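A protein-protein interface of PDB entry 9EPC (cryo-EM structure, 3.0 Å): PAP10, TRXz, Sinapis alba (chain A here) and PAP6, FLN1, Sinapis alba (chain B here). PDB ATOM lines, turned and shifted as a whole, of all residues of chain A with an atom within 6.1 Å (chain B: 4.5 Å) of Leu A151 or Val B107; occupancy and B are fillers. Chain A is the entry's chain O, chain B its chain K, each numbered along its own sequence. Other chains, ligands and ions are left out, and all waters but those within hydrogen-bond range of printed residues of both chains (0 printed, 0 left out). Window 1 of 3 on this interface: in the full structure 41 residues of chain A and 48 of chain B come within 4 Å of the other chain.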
ATOM      1  N   ASP A 102       4.223   6.838   4.230  1.00  0.00           N
ATOM      2  CA  ASP A 102       2.831   7.258   4.259  1.00  0.00           C
ATOM      3  C   ASP A 102       2.396   7.654   2.857  1.00  0.00           C
ATOM      4  O   ASP A 102       3.096   8.404   2.171  1.00  0.00           O
ATOM      5  CB  ASP A 102       2.626   8.434   5.214  1.00  0.00           C
ATOM      6  CG  ASP A 102       1.157   8.717   5.488  1.00  0.00           C
ATOM      7  OD1 ASP A 102       0.853   9.280   6.558  1.00  0.00           O
ATOM      8  OD2 ASP A 102       0.301   8.364   4.652  1.00  0.00           O
ATOM      9  N   PHE A 103       1.246   7.149   2.438  1.00  0.00           N
ATOM     10  CA  PHE A 103       0.590   7.608   1.224  1.00  0.00           C
ATOM     11  C   PHE A 103      -0.615   8.445   1.620  1.00  0.00           C
ATOM     12  O   PHE A 103      -1.433   8.015   2.437  1.00  0.00           O
ATOM     13  CB  PHE A 103       0.179   6.429   0.346  1.00  0.00           C
ATOM     14  CG  PHE A 103       1.339   5.728  -0.290  1.00  0.00           C
ATOM     15  CD1 PHE A 103       2.054   4.774   0.408  1.00  0.00           C
ATOM     16  CD2 PHE A 103       1.725   6.035  -1.580  1.00  0.00           C
ATOM     17  CE1 PHE A 103       3.125   4.136  -0.173  1.00  0.00           C
ATOM     18  CE2 PHE A 103       2.799   5.398  -2.164  1.00  0.00           C
ATOM     19  CZ  PHE A 103       3.498   4.447  -1.460  1.00  0.00           C
ATOM     20  N   TYR A 104      -0.712   9.643   1.056  1.00  0.00           N
ATOM     21  CA  TYR A 104      -1.728  10.591   1.478  1.00  0.00           C
ATOM     22  C   TYR A 104      -2.046  11.523   0.322  1.00  0.00           C
ATOM     23  O   TYR A 104      -1.323  11.586  -0.673  1.00  0.00           O
ATOM     24  CB  TYR A 104      -1.266  11.394   2.695  1.00  0.00           C
ATOM     25  CG  TYR A 104      -0.295  12.494   2.345  1.00  0.00           C
ATOM     26  CD1 TYR A 104       1.028  12.210   2.050  1.00  0.00           C
ATOM     27  CD2 TYR A 104      -0.704  13.817   2.305  1.00  0.00           C
ATOM     28  CE1 TYR A 104       1.916  13.212   1.725  1.00  0.00           C
ATOM     29  CE2 TYR A 104       0.176  14.824   1.981  1.00  0.00           C
ATOM     30  CZ  TYR A 104       1.483  14.517   1.693  1.00  0.00           C
ATOM     31  OH  TYR A 104       2.361  15.522   1.371  1.00  0.00           O
ATOM     32  N   ALA A 105      -3.147  12.250   0.469  1.00  0.00           N
ATOM     33  CA  ALA A 105      -3.508  13.315  -0.450  1.00  0.00           C
ATOM     34  C   ALA A 105      -4.040  14.486   0.357  1.00  0.00           C
ATOM     35  O   ALA A 105      -4.730  14.292   1.360  1.00  0.00           O
ATOM     36  CB  ALA A 105      -4.551  12.856  -1.469  1.00  0.00           C
ATOM     37  N   TRP A 107      -6.363  16.504  -0.319  1.00  0.00           N
ATOM     38  CA  TRP A 107      -7.819  16.549  -0.355  1.00  0.00           C
ATOM     39  C   TRP A 107      -8.471  15.461   0.480  1.00  0.00           C
ATOM     40  O   TRP A 107      -9.686  15.505   0.690  1.00  0.00           O
ATOM     41  CB  TRP A 107      -8.311  16.430  -1.796  1.00  0.00           C
ATOM     42  CG  TRP A 107      -7.832  15.203  -2.498  1.00  0.00           C
ATOM     43  CD1 TRP A 107      -6.760  15.105  -3.332  1.00  0.00           C
ATOM     44  CD2 TRP A 107      -8.398  13.890  -2.416  1.00  0.00           C
ATOM     45  NE1 TRP A 107      -6.628  13.816  -3.781  1.00  0.00           N
ATOM     46  CE2 TRP A 107      -7.620  13.051  -3.230  1.00  0.00           C
ATOM     47  CE3 TRP A 107      -9.488  13.346  -1.734  1.00  0.00           C
ATOM     48  CZ2 TRP A 107      -7.898  11.699  -3.383  1.00  0.00           C
ATOM     49  CZ3 TRP A 107      -9.760  12.005  -1.885  1.00  0.00           C
ATOM     50  CH2 TRP A 107      -8.970  11.196  -2.703  1.00  0.00           C
ATOM     51  N   CYS A 108      -7.697  14.490   0.953  1.00  0.00           N
ATOM     52  CA  CYS A 108      -8.227  13.372   1.720  1.00  0.00           C
ATOM     53  C   CYS A 108      -8.573  13.831   3.128  1.00  0.00           C
ATOM     54  O   CYS A 108      -7.715  14.357   3.842  1.00  0.00           O
ATOM     55  CB  CYS A 108      -7.208  12.238   1.751  1.00  0.00           C
ATOM     56  SG  CYS A 108      -7.250  11.181   3.208  1.00  0.00           S
ATOM     57  N   CYS A 111      -6.749  11.902   6.077  1.00  0.00           N
ATOM     58  CA  CYS A 111      -5.303  12.073   6.079  1.00  0.00           C
ATOM     59  C   CYS A 111      -4.866  13.262   6.918  1.00  0.00           C
ATOM     60  O   CYS A 111      -3.703  13.316   7.330  1.00  0.00           O
ATOM     61  CB  CYS A 111      -4.791  12.210   4.648  1.00  0.00           C
ATOM     62  SG  CYS A 111      -5.299  10.810   3.589  1.00  0.00           S
ATOM     63  N   THR A 136      -0.133  10.950  -3.100  1.00  0.00           N
ATOM     64  CA  THR A 136      -0.693  10.164  -4.190  1.00  0.00           C
ATOM     65  C   THR A 136      -1.133  11.017  -5.369  1.00  0.00           C
ATOM     66  O   THR A 136      -1.384  10.469  -6.444  1.00  0.00           O
ATOM     67  CB  THR A 136      -1.873   9.330  -3.694  1.00  0.00           C
ATOM     68  OG1 THR A 136      -2.868  10.194  -3.136  1.00  0.00           O
ATOM     69  CG2 THR A 136      -1.411   8.342  -2.640  1.00  0.00           C
ATOM     70  N   TYR A 140       0.423   8.932  -8.347  1.00  0.00           N
ATOM     71  CA  TYR A 140      -0.773   8.097  -8.398  1.00  0.00           C
ATOM     72  C   TYR A 140      -0.472   6.736  -9.011  1.00  0.00           C
ATOM     73  O   TYR A 140      -0.925   5.703  -8.508  1.00  0.00           O
ATOM     74  CB  TYR A 140      -1.871   8.814  -9.181  1.00  0.00           C
ATOM     75  CG  TYR A 140      -3.168   8.047  -9.275  1.00  0.00           C
ATOM     76  CD1 TYR A 140      -4.065   8.030  -8.219  1.00  0.00           C
ATOM     77  CD2 TYR A 140      -3.500   7.350 -10.425  1.00  0.00           C
ATOM     78  CE1 TYR A 140      -5.251   7.336  -8.303  1.00  0.00           C
ATOM     79  CE2 TYR A 140      -4.682   6.653 -10.519  1.00  0.00           C
ATOM     80  CZ  TYR A 140      -5.555   6.650  -9.456  1.00  0.00           C
ATOM     81  OH  TYR A 140      -6.736   5.954  -9.547  1.00  0.00           O
ATOM     82  N   VAL A 148      -1.891  -0.072  -3.215  1.00  0.00           N
ATOM     83  CA  VAL A 148      -2.572   0.866  -2.335  1.00  0.00           C
ATOM     84  C   VAL A 148      -4.023   0.954  -2.786  1.00  0.00           C
ATOM     85  O   VAL A 148      -4.305   1.375  -3.914  1.00  0.00           O
ATOM     86  CB  VAL A 148      -1.899   2.246  -2.356  1.00  0.00           C
ATOM     87  CG1 VAL A 148      -2.700   3.236  -1.539  1.00  0.00           C
ATOM     88  CG2 VAL A 148      -0.485   2.150  -1.824  1.00  0.00           C
ATOM     89  N   ARG A 149      -4.941   0.552  -1.913  1.00  0.00           N
ATOM     90  CA  ARG A 149      -6.359   0.538  -2.246  1.00  0.00           C
ATOM     91  C   ARG A 149      -7.110   1.749  -1.718  1.00  0.00           C
ATOM     92  O   ARG A 149      -8.110   2.154  -2.318  1.00  0.00           O
ATOM     93  CB  ARG A 149      -7.015  -0.737  -1.705  1.00  0.00           C
ATOM     94  CG  ARG A 149      -6.301  -2.013  -2.113  1.00  0.00           C
ATOM     95  CD  ARG A 149      -7.056  -3.241  -1.644  1.00  0.00           C
ATOM     96  NE  ARG A 149      -7.243  -3.250  -0.198  1.00  0.00           N
ATOM     97  CZ  ARG A 149      -7.919  -4.180   0.461  1.00  0.00           C
ATOM     98  NH1 ARG A 149      -8.488  -5.196  -0.166  1.00  0.00           N
ATOM     99  NH2 ARG A 149      -8.027  -4.089   1.783  1.00  0.00           N
ATOM    100  N   GLY A 150      -6.655   2.333  -0.610  1.00  0.00           N
ATOM    101  CA  GLY A 150      -7.276   3.521  -0.070  1.00  0.00           C
ATOM    102  C   GLY A 150      -6.216   4.498   0.396  1.00  0.00           C
ATOM    103  O   GLY A 150      -5.028   4.178   0.442  1.00  0.00           O
ATOM    104  N   LEU A 151      -6.665   5.691   0.751  1.00  0.00           N
ATOM    105  CA  LEU A 151      -5.703   6.759   0.977  1.00  0.00           C
ATOM    106  C   LEU A 151      -4.970   6.622   2.308  1.00  0.00           C
ATOM    107  O   LEU A 151      -3.734   6.620   2.310  1.00  0.00           O
ATOM    108  CB  LEU A 151      -6.381   8.123   0.871  1.00  0.00           C
ATOM    109  CG  LEU A 151      -5.480   9.234   0.338  1.00  0.00           C
ATOM    110  CD1 LEU A 151      -4.279   8.675  -0.400  1.00  0.00           C
ATOM    111  CD2 LEU A 151      -6.287  10.117  -0.577  1.00  0.00           C
ATOM    112  N   PRO A 152      -5.655   6.497   3.460  1.00  0.00           N
ATOM    113  CA  PRO A 152      -4.901   6.388   4.717  1.00  0.00           C
ATOM    114  C   PRO A 152      -4.164   5.063   4.810  1.00  0.00           C
ATOM    115  O   PRO A 152      -4.576   4.162   5.546  1.00  0.00           O
ATOM    116  CB  PRO A 152      -5.984   6.510   5.798  1.00  0.00           C
ATOM    117  CG  PRO A 152      -7.186   7.045   5.095  1.00  0.00           C
ATOM    118  CD  PRO A 152      -7.104   6.502   3.713  1.00  0.00           C
ATOM    119  N   THR A 153      -3.070   4.938   4.062  1.00  0.00           N
ATOM    120  CA  THR A 153      -2.325   3.692   3.952  1.00  0.00           C
ATOM    121  C   THR A 153      -0.860   3.944   4.268  1.00  0.00           C
ATOM    122  O   THR A 153      -0.264   4.888   3.740  1.00  0.00           O
ATOM    123  CB  THR A 153      -2.464   3.094   2.551  1.00  0.00           C
ATOM    124  OG1 THR A 153      -3.844   2.815   2.285  1.00  0.00           O
ATOM    125  CG2 THR A 153      -1.667   1.814   2.435  1.00  0.00           C
ATOM    126  N   LEU A 154      -0.285   3.104   5.122  1.00  0.00           N
ATOM    127  CA  LEU A 154       1.122   3.178   5.478  1.00  0.00           C
ATOM    128  C   LEU A 154       1.838   1.912   5.033  1.00  0.00           C
ATOM    129  O   LEU A 154       1.217   0.883   4.758  1.00  0.00           O
ATOM    130  CB  LEU A 154       1.319   3.368   6.987  1.00  0.00           C
ATOM    131  CG  LEU A 154       0.639   4.558   7.661  1.00  0.00           C
ATOM    132  CD1 LEU A 154      -0.739   4.171   8.160  1.00  0.00           C
ATOM    133  CD2 LEU A 154       1.493   5.079   8.797  1.00  0.00           C
ATOM    134  N   GLU A 169      -3.978  -0.119   6.587  1.00  0.00           N
ATOM    135  CA  GLU A 169      -4.956   0.734   5.928  1.00  0.00           C
ATOM    136  C   GLU A 169      -5.922   1.295   6.958  1.00  0.00           C
ATOM    137  O   GLU A 169      -6.435   0.554   7.802  1.00  0.00           O
ATOM    138  CB  GLU A 169      -5.720  -0.034   4.848  1.00  0.00           C
ATOM    139  CG  GLU A 169      -4.826  -0.780   3.876  1.00  0.00           C
ATOM    140  CD  GLU A 169      -5.324  -0.709   2.448  1.00  0.00           C
ATOM    141  OE1 GLU A 169      -4.865   0.180   1.701  1.00  0.00           O
ATOM    142  OE2 GLU A 169      -6.177  -1.540   2.072  1.00  0.00           O
ATOM    143  N   VAL B 104     -11.028   6.225   3.174  1.00  0.00           N
ATOM    144  CA  VAL B 104     -11.758   6.495   1.938  1.00  0.00           C
ATOM    145  C   VAL B 104     -11.145   5.666   0.814  1.00  0.00           C
ATOM    146  O   VAL B 104      -9.945   5.790   0.534  1.00  0.00           O
ATOM    147  CB  VAL B 104     -11.754   7.995   1.602  1.00  0.00           C
ATOM    148  CG1 VAL B 104     -10.374   8.589   1.817  1.00  0.00           C
ATOM    149  CG2 VAL B 104     -12.218   8.217   0.173  1.00  0.00           C
ATOM    150  N   PRO B 105     -11.918   4.801   0.156  1.00  0.00           N
ATOM    151  CA  PRO B 105     -11.345   3.960  -0.903  1.00  0.00           C
ATOM    152  C   PRO B 105     -11.189   4.672  -2.238  1.00  0.00           C
ATOM    153  O   PRO B 105     -10.216   4.428  -2.957  1.00  0.00           O
ATOM    154  CB  PRO B 105     -12.349   2.806  -1.003  1.00  0.00           C
ATOM    155  CG  PRO B 105     -13.634   3.406  -0.582  1.00  0.00           C
ATOM    156  CD  PRO B 105     -13.304   4.420   0.475  1.00  0.00           C
ATOM    157  N   VAL B 106     -12.126   5.552  -2.581  1.00  0.00           N
ATOM    158  CA  VAL B 106     -12.114   6.201  -3.889  1.00  0.00           C
ATOM    159  C   VAL B 106     -10.976   7.217  -3.913  1.00  0.00           C
ATOM    160  O   VAL B 106     -11.071   8.283  -3.300  1.00  0.00           O
ATOM    161  CB  VAL B 106     -13.457   6.867  -4.203  1.00  0.00           C
ATOM    162  CG1 VAL B 106     -13.381   7.602  -5.527  1.00  0.00           C
ATOM    163  CG2 VAL B 106     -14.565   5.834  -4.231  1.00  0.00           C
ATOM    164  N   VAL B 107      -9.901   6.892  -4.624  1.00  0.00           N
ATOM    165  CA  VAL B 107      -8.731   7.753  -4.722  1.00  0.00           C
ATOM    166  C   VAL B 107      -8.416   7.980  -6.192  1.00  0.00           C
ATOM    167  O   VAL B 107      -8.250   7.019  -6.951  1.00  0.00           O
ATOM    168  CB  VAL B 107      -7.513   7.145  -4.003  1.00  0.00           C
ATOM    169  CG1 VAL B 107      -6.305   8.050  -4.157  1.00  0.00           C
ATOM    170  CG2 VAL B 107      -7.827   6.914  -2.538  1.00  0.00           C
ATOM    171  N   ARG B 108      -8.336   9.246  -6.591  1.00  0.00           N
ATOM    172  CA  ARG B 108      -7.947   9.614  -7.944  1.00  0.00           C
ATOM    173  C   ARG B 108      -6.953  10.763  -7.867  1.00  0.00           C
ATOM    174  O   ARG B 108      -6.750  11.368  -6.812  1.00  0.00           O
ATOM    175  CB  ARG B 108      -9.157  10.005  -8.799  1.00  0.00           C
ATOM    176  CG  ARG B 108     -10.278   8.986  -8.790  1.00  0.00           C
ATOM    177  CD  ARG B 108     -11.305   9.287  -9.859  1.00  0.00           C
ATOM    178  NE  ARG B 108     -10.772   9.055 -11.195  1.00  0.00           N
ATOM    179  CZ  ARG B 108     -11.465   9.208 -12.313  1.00  0.00           C
ATOM    180  NH1 ARG B 108     -12.727   9.605 -12.295  1.00  0.00           N
ATOM    181  NH2 ARG B 108     -10.879   8.957 -13.479  1.00  0.00           N
ATOM    182  N   LEU B 272      -8.647   2.489  -5.407  1.00  0.00           N
ATOM    183  CA  LEU B 272      -7.617   3.009  -6.304  1.00  0.00           C
ATOM    184  C   LEU B 272      -7.276   2.075  -7.461  1.00  0.00           C
ATOM    185  O   LEU B 272      -7.186   2.559  -8.600  1.00  0.00           O
ATOM    186  CB  LEU B 272      -6.372   3.351  -5.473  1.00  0.00           C
ATOM    187  CG  LEU B 272      -5.441   4.466  -5.951  1.00  0.00           C
ATOM    188  CD1 LEU B 272      -4.535   4.897  -4.815  1.00  0.00           C
ATOM    189  CD2 LEU B 272      -4.611   4.027  -7.139  1.00  0.00           C
ATOM    190  N   TRP B 275      -9.675   2.091 -10.769  1.00  0.00           N
ATOM    191  CA  TRP B 275      -9.782   3.251 -11.641  1.00  0.00           C
ATOM    192  C   TRP B 275      -8.787   3.217 -12.791  1.00  0.00           C
ATOM    193  O   TRP B 275      -8.728   4.175 -13.567  1.00  0.00           O
ATOM    194  CB  TRP B 275      -9.581   4.541 -10.840  1.00  0.00           C
ATOM    195  CG  TRP B 275     -10.687   4.841  -9.884  1.00  0.00           C
ATOM    196  CD1 TRP B 275     -10.713   4.565  -8.552  1.00  0.00           C
ATOM    197  CD2 TRP B 275     -11.929   5.483 -10.186  1.00  0.00           C
ATOM    198  NE1 TRP B 275     -11.895   4.992  -8.003  1.00  0.00           N
ATOM    199  CE2 TRP B 275     -12.659   5.560  -8.987  1.00  0.00           C
ATOM    200  CE3 TRP B 275     -12.493   5.999 -11.354  1.00  0.00           C
ATOM    201  CZ2 TRP B 275     -13.923   6.131  -8.924  1.00  0.00           C
ATOM    202  CZ3 TRP B 275     -13.748   6.565 -11.286  1.00  0.00           C
ATOM    203  CH2 TRP B 275     -14.449   6.626 -10.081  1.00  0.00           C
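O of Arg A149 sits close to O of Pro B105 (3.2 Å). The backbone carbonyl oxygen of Val B104 is in hydrogen-bond range of the backbone NH of Leu A151. N of Leu B272 sits at hydrogen-bond distance from O of Arg A149, at 3.2 Å. OH of Tyr A140 sits at hydrogen-bond distance from O of Val B107.
O of Phe A103 lies close to O of Leu A151. The guanidinium group (NE) of Arg A149 is in salt-bridge range of the side-chain carboxylate (OE2) of Glu A169. The backbone carbonyl oxygen (O) of Gly A150 sits at hydrogen-bond distance from the side-chain hydroxyl (OG1) of Thr A153 (2.6 Å). SG of Cys A108 is disulfide-bonded to SG of Cys A111, 2.0 Å away. The backbone carbonyl oxygen of Pro B105 lies within hydrogen-bond range of the backbone NH of Leu B272, 3.5 Å away.
Trp A107 touches Val B106 (CH2 to O, 3.6 Å). CH2 of Trp A107 touches CA of Val B107 (3.998 Å). Arg B108 touches Trp A107 (O to CZ2, 3.6 Å). CA of Arg B108 touches CE1 of Tyr A140, at 3.5 Å. Tyr A140 touches Leu B272 (OH to O, 3.6 Å). Tyr A140 touches Trp B275. Val A148 touches Leu B272 (O to CB, 3.3 Å). Gly A150 touches Val B104 (CA to O, 3.6 Å). N of Leu A151 touches CG2 of Val B107 (3.7 Å). Pro A152 touches Val B104.
Tyr A104 touches none of the printed residues of chain B. Printed residues of chain B within 4 Å of Trp A107: Val B106, Val B107 and Arg B108. Cys A111 touches none of the printed residues of chain B. Of the printed residues of chain B, Val A148 touches Leu B272. Of the printed residues of chain B, Arg A149 touches Pro B105 (3.2 Å) and Leu B272 (3.2 Å). Of chain B, only Val B104 and Val B107 come within 4 Å of Leu A151. Printed residues of chain A within 4 Å of Pro B105: Arg A149. Printed residues of chain A within 4 Å of Val B106: Trp A107 (3.6 Å). Of the printed residues of chain A, Val B107 touches Trp A107 (3.998 Å), Tyr A140 (3.2 Å) and Leu A151 (3.7 Å). The nearest printed residue of chain B that does not touch Trp A107 is Val B104 (5.0 Å).
Of the 7 printed residues of chain B, 7 touch a printed residue of chain A. Printed residues of chain B that touch a printed residue of chain A: Val B104, Pro B105, Val B106, Val B107, Arg B108, Leu B272 and Trp B275. Hydrophobic or aromatic side chains of chain B that line the printed part of chain A: Val B107, Leu B272 and Trp B275. Among the printed residues, 14 pairs touch across the chains. Among the printed residues, no Asp or Glu carboxylate lies within 4 Å of a Lys or Arg side-chain nitrogen of the other chain.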
